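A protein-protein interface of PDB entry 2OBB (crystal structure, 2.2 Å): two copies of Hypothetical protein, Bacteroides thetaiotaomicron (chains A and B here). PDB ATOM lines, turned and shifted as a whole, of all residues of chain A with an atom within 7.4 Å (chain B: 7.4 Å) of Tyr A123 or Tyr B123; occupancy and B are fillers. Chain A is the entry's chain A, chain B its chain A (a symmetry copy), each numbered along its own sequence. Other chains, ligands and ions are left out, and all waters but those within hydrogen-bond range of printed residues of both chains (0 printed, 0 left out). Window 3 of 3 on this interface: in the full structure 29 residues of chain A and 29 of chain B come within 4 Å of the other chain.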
ATOM      1  N   PRO A 104      -1.972  -7.610  28.135  1.00  0.00           N
ATOM      2  CA  PRO A 104      -0.857  -7.685  27.194  1.00  0.00           C
ATOM      3  C   PRO A 104       0.248  -8.436  27.929  1.00  0.00           C
ATOM      4  O   PRO A 104       0.070  -8.837  29.071  1.00  0.00           O
ATOM      5  CB  PRO A 104      -0.502  -6.215  26.960  1.00  0.00           C
ATOM      6  CG  PRO A 104      -0.883  -5.541  28.270  1.00  0.00           C
ATOM      7  CD  PRO A 104      -1.932  -6.380  28.954  1.00  0.00           C
ATOM      8  N   ASP A 105       1.381  -8.664  27.303  1.00  0.00           N
ATOM      9  CA  ASP A 105       2.393  -9.376  28.042  1.00  0.00           C
ATOM     10  C   ASP A 105       2.983  -8.502  29.157  1.00  0.00           C
ATOM     11  O   ASP A 105       2.828  -7.242  29.182  1.00  0.00           O
ATOM     12  CB  ASP A 105       3.450  -9.937  27.108  1.00  0.00           C
ATOM     13  CG  ASP A 105       4.087  -8.879  26.277  1.00  0.00           C
ATOM     14  OD1 ASP A 105       4.508  -7.857  26.859  1.00  0.00           O
ATOM     15  OD2 ASP A 105       4.193  -9.081  25.038  1.00  0.00           O
ATOM     16  N   ILE A 108       4.594  -5.098  28.840  1.00  0.00           N
ATOM     17  CA  ILE A 108       3.743  -3.954  28.670  1.00  0.00           C
ATOM     18  C   ILE A 108       3.016  -3.622  29.972  1.00  0.00           C
ATOM     19  O   ILE A 108       2.858  -2.455  30.300  1.00  0.00           O
ATOM     20  CB  ILE A 108       2.774  -4.086  27.472  1.00  0.00           C
ATOM     21  CG1 ILE A 108       3.522  -3.867  26.159  1.00  0.00           C
ATOM     22  CG2 ILE A 108       1.737  -2.949  27.487  1.00  0.00           C
ATOM     23  CD1 ILE A 108       3.879  -5.119  25.445  1.00  0.00           C
ATOM     24  N   MET A 112       3.277   0.056  31.634  1.00  0.00           N
ATOM     25  CA  MET A 112       2.050   0.822  31.905  1.00  0.00           C
ATOM     26  C   MET A 112       1.983   1.320  33.363  1.00  0.00           C
ATOM     27  O   MET A 112       1.693   2.498  33.618  1.00  0.00           O
ATOM     28  CB  MET A 112       0.811  -0.009  31.569  1.00  0.00           C
ATOM     29  CG  MET A 112       0.687  -0.386  30.113  1.00  0.00           C
ATOM     30  SD  MET A 112      -0.995  -1.353  29.730  1.00  0.00           S
ATOM     31  CE  MET A 112      -0.933  -2.815  30.949  1.00  0.00           C
ATOM     32  N   THR A 118      -1.705   4.146  29.527  1.00  0.00           N
ATOM     33  CA  THR A 118      -2.900   3.436  29.116  1.00  0.00           C
ATOM     34  C   THR A 118      -2.535   2.666  27.864  1.00  0.00           C
ATOM     35  O   THR A 118      -1.496   2.927  27.262  1.00  0.00           O
ATOM     36  CB  THR A 118      -4.027   4.440  28.752  1.00  0.00           C
ATOM     37  OG1 THR A 118      -3.552   5.337  27.745  1.00  0.00           O
ATOM     38  CG2 THR A 118      -4.460   5.256  29.962  1.00  0.00           C
ATOM     39  N   PHE A 119      -3.387   1.724  27.458  1.00  0.00           N
ATOM     40  CA  PHE A 119      -3.182   1.056  26.182  1.00  0.00           C
ATOM     41  C   PHE A 119      -3.063   2.144  25.121  1.00  0.00           C
ATOM     42  O   PHE A 119      -2.247   2.041  24.198  1.00  0.00           O
ATOM     43  CB  PHE A 119      -4.344   0.125  25.863  1.00  0.00           C
ATOM     44  CG  PHE A 119      -4.349  -1.162  26.671  1.00  0.00           C
ATOM     45  CD1 PHE A 119      -3.633  -2.276  26.238  1.00  0.00           C
ATOM     46  CD2 PHE A 119      -5.081  -1.258  27.838  1.00  0.00           C
ATOM     47  CE1 PHE A 119      -3.656  -3.467  26.947  1.00  0.00           C
ATOM     48  CE2 PHE A 119      -5.097  -2.438  28.568  1.00  0.00           C
ATOM     49  CZ  PHE A 119      -4.386  -3.557  28.110  1.00  0.00           C
ATOM     50  N   ALA A 120      -3.846   3.205  25.281  1.00  0.00           N
ATOM     51  CA  ALA A 120      -3.880   4.301  24.299  1.00  0.00           C
ATOM     52  C   ALA A 120      -2.482   4.880  24.116  1.00  0.00           C
ATOM     53  O   ALA A 120      -1.963   4.923  22.997  1.00  0.00           O
ATOM     54  CB  ALA A 120      -4.869   5.372  24.719  1.00  0.00           C
ATOM     55  N   ASP A 121      -1.865   5.282  25.228  1.00  0.00           N
ATOM     56  CA  ASP A 121      -0.464   5.730  25.254  1.00  0.00           C
ATOM     57  C   ASP A 121       0.480   4.738  24.597  1.00  0.00           C
ATOM     58  O   ASP A 121       1.184   5.105  23.671  1.00  0.00           O
ATOM     59  CB  ASP A 121      -0.005   5.963  26.687  1.00  0.00           C
ATOM     60  CG  ASP A 121      -0.815   7.014  27.390  1.00  0.00           C
ATOM     61  OD1 ASP A 121      -1.354   7.915  26.705  1.00  0.00           O
ATOM     62  OD2 ASP A 121      -0.912   6.942  28.628  1.00  0.00           O
ATOM     63  N   ILE A 122       0.482   3.491  25.079  1.00  0.00           N
ATOM     64  CA  ILE A 122       1.341   2.436  24.555  1.00  0.00           C
ATOM     65  C   ILE A 122       1.298   2.406  23.039  1.00  0.00           C
ATOM     66  O   ILE A 122       2.336   2.485  22.381  1.00  0.00           O
ATOM     67  CB  ILE A 122       0.933   1.041  25.099  1.00  0.00           C
ATOM     68  CG1 ILE A 122       1.119   0.959  26.616  1.00  0.00           C
ATOM     69  CG2 ILE A 122       1.705  -0.088  24.383  1.00  0.00           C
ATOM     70  CD1 ILE A 122       2.560   1.023  27.091  1.00  0.00           C
ATOM     71  N   TYR A 123       0.095   2.335  22.483  1.00  0.00           N
ATOM     72  CA  TYR A 123      -0.045   2.214  21.041  1.00  0.00           C
ATOM     73  C   TYR A 123       0.160   3.510  20.242  1.00  0.00           C
ATOM     74  O   TYR A 123       0.700   3.455  19.124  1.00  0.00           O
ATOM     75  CB  TYR A 123      -1.333   1.473  20.672  1.00  0.00           C
ATOM     76  CG  TYR A 123      -1.295   0.022  21.129  1.00  0.00           C
ATOM     77  CD1 TYR A 123      -0.624  -0.954  20.383  1.00  0.00           C
ATOM     78  CD2 TYR A 123      -1.903  -0.371  22.316  1.00  0.00           C
ATOM     79  CE1 TYR A 123      -0.572  -2.299  20.813  1.00  0.00           C
ATOM     80  CE2 TYR A 123      -1.861  -1.704  22.753  1.00  0.00           C
ATOM     81  CZ  TYR A 123      -1.198  -2.661  21.996  1.00  0.00           C
ATOM     82  OH  TYR A 123      -1.154  -3.973  22.433  1.00  0.00           O
ATOM     83  N   SER A 124      -0.219   4.665  20.799  1.00  0.00           N
ATOM     84  CA  SER A 124      -0.046   5.929  20.054  1.00  0.00           C
ATOM     85  C   SER A 124       1.430   6.353  19.854  1.00  0.00           C
ATOM     86  O   SER A 124       2.214   6.452  20.804  1.00  0.00           O
ATOM     87  CB  SER A 124      -0.964   7.073  20.564  1.00  0.00           C
ATOM     88  OG  SER A 124      -0.595   7.598  21.833  1.00  0.00           O
ATOM     89  N   GLN A 125       1.781   6.588  18.589  1.00  0.00           N
ATOM     90  CA  GLN A 125       3.161   6.851  18.153  1.00  0.00           C
ATOM     91  C   GLN A 125       3.304   8.180  17.382  1.00  0.00           C
ATOM     92  O   GLN A 125       4.109   8.298  16.441  1.00  0.00           O
ATOM     93  CB  GLN A 125       3.661   5.681  17.290  1.00  0.00           C
ATOM     94  CG  GLN A 125       2.916   5.516  15.953  1.00  0.00           C
ATOM     95  CD  GLN A 125       2.672   4.063  15.594  1.00  0.00           C
ATOM     96  OE1 GLN A 125       2.552   3.200  16.478  1.00  0.00           O
ATOM     97  NE2 GLN A 125       2.594   3.783  14.293  1.00  0.00           N
ATOM     98  N   PRO B 104     -11.284   1.879  27.850  1.00  0.00           N
ATOM     99  CA  PRO B 104     -11.449   2.824  26.749  1.00  0.00           C
ATOM    100  C   PRO B 104     -12.914   3.246  26.789  1.00  0.00           C
ATOM    101  O   PRO B 104     -13.664   2.795  27.643  1.00  0.00           O
ATOM    102  CB  PRO B 104     -11.122   1.980  25.516  1.00  0.00           C
ATOM    103  CG  PRO B 104     -11.539   0.574  25.922  1.00  0.00           C
ATOM    104  CD  PRO B 104     -11.508   0.481  27.426  1.00  0.00           C
ATOM    105  N   ASP B 105     -13.345   4.117  25.905  1.00  0.00           N
ATOM    106  CA  ASP B 105     -14.737   4.480  25.984  1.00  0.00           C
ATOM    107  C   ASP B 105     -15.639   3.321  25.538  1.00  0.00           C
ATOM    108  O   ASP B 105     -15.191   2.329  24.883  1.00  0.00           O
ATOM    109  CB  ASP B 105     -15.005   5.765  25.220  1.00  0.00           C
ATOM    110  CG  ASP B 105     -14.592   5.670  23.793  1.00  0.00           C
ATOM    111  OD1 ASP B 105     -14.981   4.678  23.141  1.00  0.00           O
ATOM    112  OD2 ASP B 105     -13.898   6.605  23.313  1.00  0.00           O
ATOM    113  N   ILE B 108     -15.575   1.453  22.253  1.00  0.00           N
ATOM    114  CA  ILE B 108     -14.550   0.468  22.049  1.00  0.00           C
ATOM    115  C   ILE B 108     -14.820  -0.778  22.891  1.00  0.00           C
ATOM    116  O   ILE B 108     -14.598  -1.886  22.425  1.00  0.00           O
ATOM    117  CB  ILE B 108     -13.121   1.022  22.259  1.00  0.00           C
ATOM    118  CG1 ILE B 108     -12.702   1.872  21.061  1.00  0.00           C
ATOM    119  CG2 ILE B 108     -12.092  -0.123  22.261  1.00  0.00           C
ATOM    120  CD1 ILE B 108     -12.829   3.336  21.280  1.00  0.00           C
ATOM    121  N   MET B 112     -15.062  -4.439  21.189  1.00  0.00           N
ATOM    122  CA  MET B 112     -14.178  -5.519  21.655  1.00  0.00           C
ATOM    123  C   MET B 112     -14.961  -6.796  22.023  1.00  0.00           C
ATOM    124  O   MET B 112     -14.596  -7.906  21.608  1.00  0.00           O
ATOM    125  CB  MET B 112     -13.335  -5.051  22.842  1.00  0.00           C
ATOM    126  CG  MET B 112     -12.387  -3.919  22.527  1.00  0.00           C
ATOM    127  SD  MET B 112     -11.245  -3.447  24.071  1.00  0.00           S
ATOM    128  CE  MET B 112     -12.513  -3.090  25.447  1.00  0.00           C
ATOM    129  N   THR B 118      -9.060  -7.593  21.101  1.00  0.00           N
ATOM    130  CA  THR B 118      -8.162  -7.156  22.153  1.00  0.00           C
ATOM    131  C   THR B 118      -7.800  -5.719  21.841  1.00  0.00           C
ATOM    132  O   THR B 118      -8.043  -5.251  20.731  1.00  0.00           O
ATOM    133  CB  THR B 118      -6.857  -7.997  22.134  1.00  0.00           C
ATOM    134  OG1 THR B 118      -6.261  -7.911  20.837  1.00  0.00           O
ATOM    135  CG2 THR B 118      -7.132  -9.461  22.445  1.00  0.00           C
ATOM    136  N   PHE B 119      -7.209  -5.016  22.807  1.00  0.00           N
ATOM    137  CA  PHE B 119      -6.691  -3.685  22.529  1.00  0.00           C
ATOM    138  C   PHE B 119      -5.759  -3.809  21.329  1.00  0.00           C
ATOM    139  O   PHE B 119      -5.738  -2.940  20.452  1.00  0.00           O
ATOM    140  CB  PHE B 119      -5.941  -3.132  23.732  1.00  0.00           C
ATOM    141  CG  PHE B 119      -6.839  -2.674  24.868  1.00  0.00           C
ATOM    142  CD1 PHE B 119      -7.361  -1.382  24.885  1.00  0.00           C
ATOM    143  CD2 PHE B 119      -7.138  -3.522  25.916  1.00  0.00           C
ATOM    144  CE1 PHE B 119      -8.155  -0.940  25.932  1.00  0.00           C
ATOM    145  CE2 PHE B 119      -7.947  -3.099  26.961  1.00  0.00           C
ATOM    146  CZ  PHE B 119      -8.450  -1.789  26.974  1.00  0.00           C
ATOM    147  N   ALA B 120      -5.023  -4.915  21.272  1.00  0.00           N
ATOM    148  CA  ALA B 120      -4.036  -5.136  20.203  1.00  0.00           C
ATOM    149  C   ALA B 120      -4.715  -5.056  18.841  1.00  0.00           C
ATOM    150  O   ALA B 120      -4.318  -4.258  17.988  1.00  0.00           O
ATOM    151  CB  ALA B 120      -3.329  -6.465  20.389  1.00  0.00           C
ATOM    152  N   ASP B 121      -5.767  -5.857  18.664  1.00  0.00           N
ATOM    153  CA  ASP B 121      -6.625  -5.807  17.470  1.00  0.00           C
ATOM    154  C   ASP B 121      -7.121  -4.405  17.164  1.00  0.00           C
ATOM    155  O   ASP B 121      -6.887  -3.912  16.073  1.00  0.00           O
ATOM    156  CB  ASP B 121      -7.829  -6.724  17.640  1.00  0.00           C
ATOM    157  CG  ASP B 121      -7.439  -8.159  17.840  1.00  0.00           C
ATOM    158  OD1 ASP B 121      -6.356  -8.561  17.354  1.00  0.00           O
ATOM    159  OD2 ASP B 121      -8.216  -8.889  18.482  1.00  0.00           O
ATOM    160  N   ILE B 122      -7.797  -3.775  18.131  1.00  0.00           N
ATOM    161  CA  ILE B 122      -8.341  -2.431  17.978  1.00  0.00           C
ATOM    162  C   ILE B 122      -7.311  -1.497  17.372  1.00  0.00           C
ATOM    163  O   ILE B 122      -7.568  -0.859  16.350  1.00  0.00           O
ATOM    164  CB  ILE B 122      -8.817  -1.847  19.334  1.00  0.00           C
ATOM    165  CG1 ILE B 122      -9.978  -2.659  19.914  1.00  0.00           C
ATOM    166  CG2 ILE B 122      -9.194  -0.355  19.201  1.00  0.00           C
ATOM    167  CD1 ILE B 122     -11.271  -2.587  19.120  1.00  0.00           C
ATOM    168  N   TYR B 123      -6.131  -1.446  17.976  1.00  0.00           N
ATOM    169  CA  TYR B 123      -5.109  -0.517  17.522  1.00  0.00           C
ATOM    170  C   TYR B 123      -4.351  -0.930  16.251  1.00  0.00           C
ATOM    171  O   TYR B 123      -3.996  -0.055  15.443  1.00  0.00           O
ATOM    172  CB  TYR B 123      -4.184  -0.109  18.672  1.00  0.00           C
ATOM    173  CG  TYR B 123      -4.926   0.697  19.728  1.00  0.00           C
ATOM    174  CD1 TYR B 123      -5.170   2.064  19.556  1.00  0.00           C
ATOM    175  CD2 TYR B 123      -5.407   0.092  20.884  1.00  0.00           C
ATOM    176  CE1 TYR B 123      -5.873   2.812  20.527  1.00  0.00           C
ATOM    177  CE2 TYR B 123      -6.105   0.823  21.857  1.00  0.00           C
ATOM    178  CZ  TYR B 123      -6.330   2.181  21.674  1.00  0.00           C
ATOM    179  OH  TYR B 123      -7.024   2.897  22.632  1.00  0.00           O
ATOM    180  N   SER B 124      -4.132  -2.233  16.038  1.00  0.00           N
ATOM    181  CA  SER B 124      -3.398  -2.664  14.832  1.00  0.00           C
ATOM    182  C   SER B 124      -4.164  -2.437  13.505  1.00  0.00           C
ATOM    183  O   SER B 124      -5.309  -2.867  13.332  1.00  0.00           O
ATOM    184  CB  SER B 124      -2.779  -4.082  14.964  1.00  0.00           C
ATOM    185  OG  SER B 124      -3.728  -5.140  14.945  1.00  0.00           O
ATOM    186  N   GLN B 125      -3.498  -1.740  12.583  1.00  0.00           N
ATOM    187  CA  GLN B 125      -4.086  -1.277  11.317  1.00  0.00           C
ATOM    188  C   GLN B 125      -3.296  -1.750  10.079  1.00  0.00           C
ATOM    189  O   GLN B 125      -3.192  -1.035   9.066  1.00  0.00           O
ATOM    190  CB  GLN B 125      -4.190   0.257  11.327  1.00  0.00           C
ATOM    191  CG  GLN B 125      -2.832   0.983  11.347  1.00  0.00           C
ATOM    192  CD  GLN B 125      -2.837   2.207  12.241  1.00  0.00           C
ATOM    193  OE1 GLN B 125      -3.587   2.273  13.228  1.00  0.00           O
ATOM    194  NE2 GLN B 125      -1.997   3.187  11.904  1.00  0.00           N
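OG1 of Thr A118 lies close to N of Ala A120 (3.3 Å).
The backbone carbonyl oxygen (O) of Ala B120 sits at hydrogen-bond distance from the side-chain hydroxyl (OG) of Ser B124.
OG of Ser A124 is in hydrogen-bond range of O of Ala A120 (3.2 Å).
The side-chain hydroxyl of Thr B118 sits close to the backbone NH of Ala B120 (3.3 Å).
The backbone carbonyl oxygen (O) of Tyr A123 sits close to the side-chain amide oxygen (OE1) of Gln A125 (3.2 Å).
The backbone carbonyl oxygen (O) of Tyr B123 sits close to the side-chain amide oxygen (OE1) of Gln B125, 3.2 Å away.
CE2 of Phe B119 touches CE2 of Phe A119, 3.3 Å away.
Ala A120 touches Tyr B123 (CA to OH, 3.8 Å).
Ala B120 touches Tyr A123.
Tyr B123 touches Tyr A123 (CB to CG, 3.8 Å).
Printed residues of chain B within 4 Å of Tyr A123: Ala B120 (3.8 Å) and Tyr B123 (3.8 Å).
Tyr B123 touches two residues of chain A.
Of the printed residues of chain B, Phe A119 touches Phe B119.
Printed residues of chain B within 4 Å of Ala A120: Tyr B123.
Of the printed residues of chain A, Ala B120 touches Tyr A123.
Printed residues of chain A within 4 Å of Phe B119: Phe A119.
The nearest residue of chain A that does not touch Tyr B123 is Phe A119 (4.4 Å).
Printed residues of chain A that touch a printed residue of chain B: Phe A119, Ala A120 and Tyr A123.
Hydrophobic or aromatic side chains of chain A within 4 Å of the printed part of chain B: Phe A119, Ala A120 and Tyr A123.
Among the printed residues, no Asp or Glu carboxylate lies within 4 Å of a Lys or Arg side-chain nitrogen of the other chain.
Phe A119 touches its own counterpart, Phe B119.
Ala A120 touches Tyr B123, and with the chains exchanged Tyr A123 touches Ala B120.
Tyr B123 touches its own counterpart, Tyr A123.
Of the 4 pairs that touch across the chains among the printed residues, 4 have their exchanged pair printed and touching as well.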
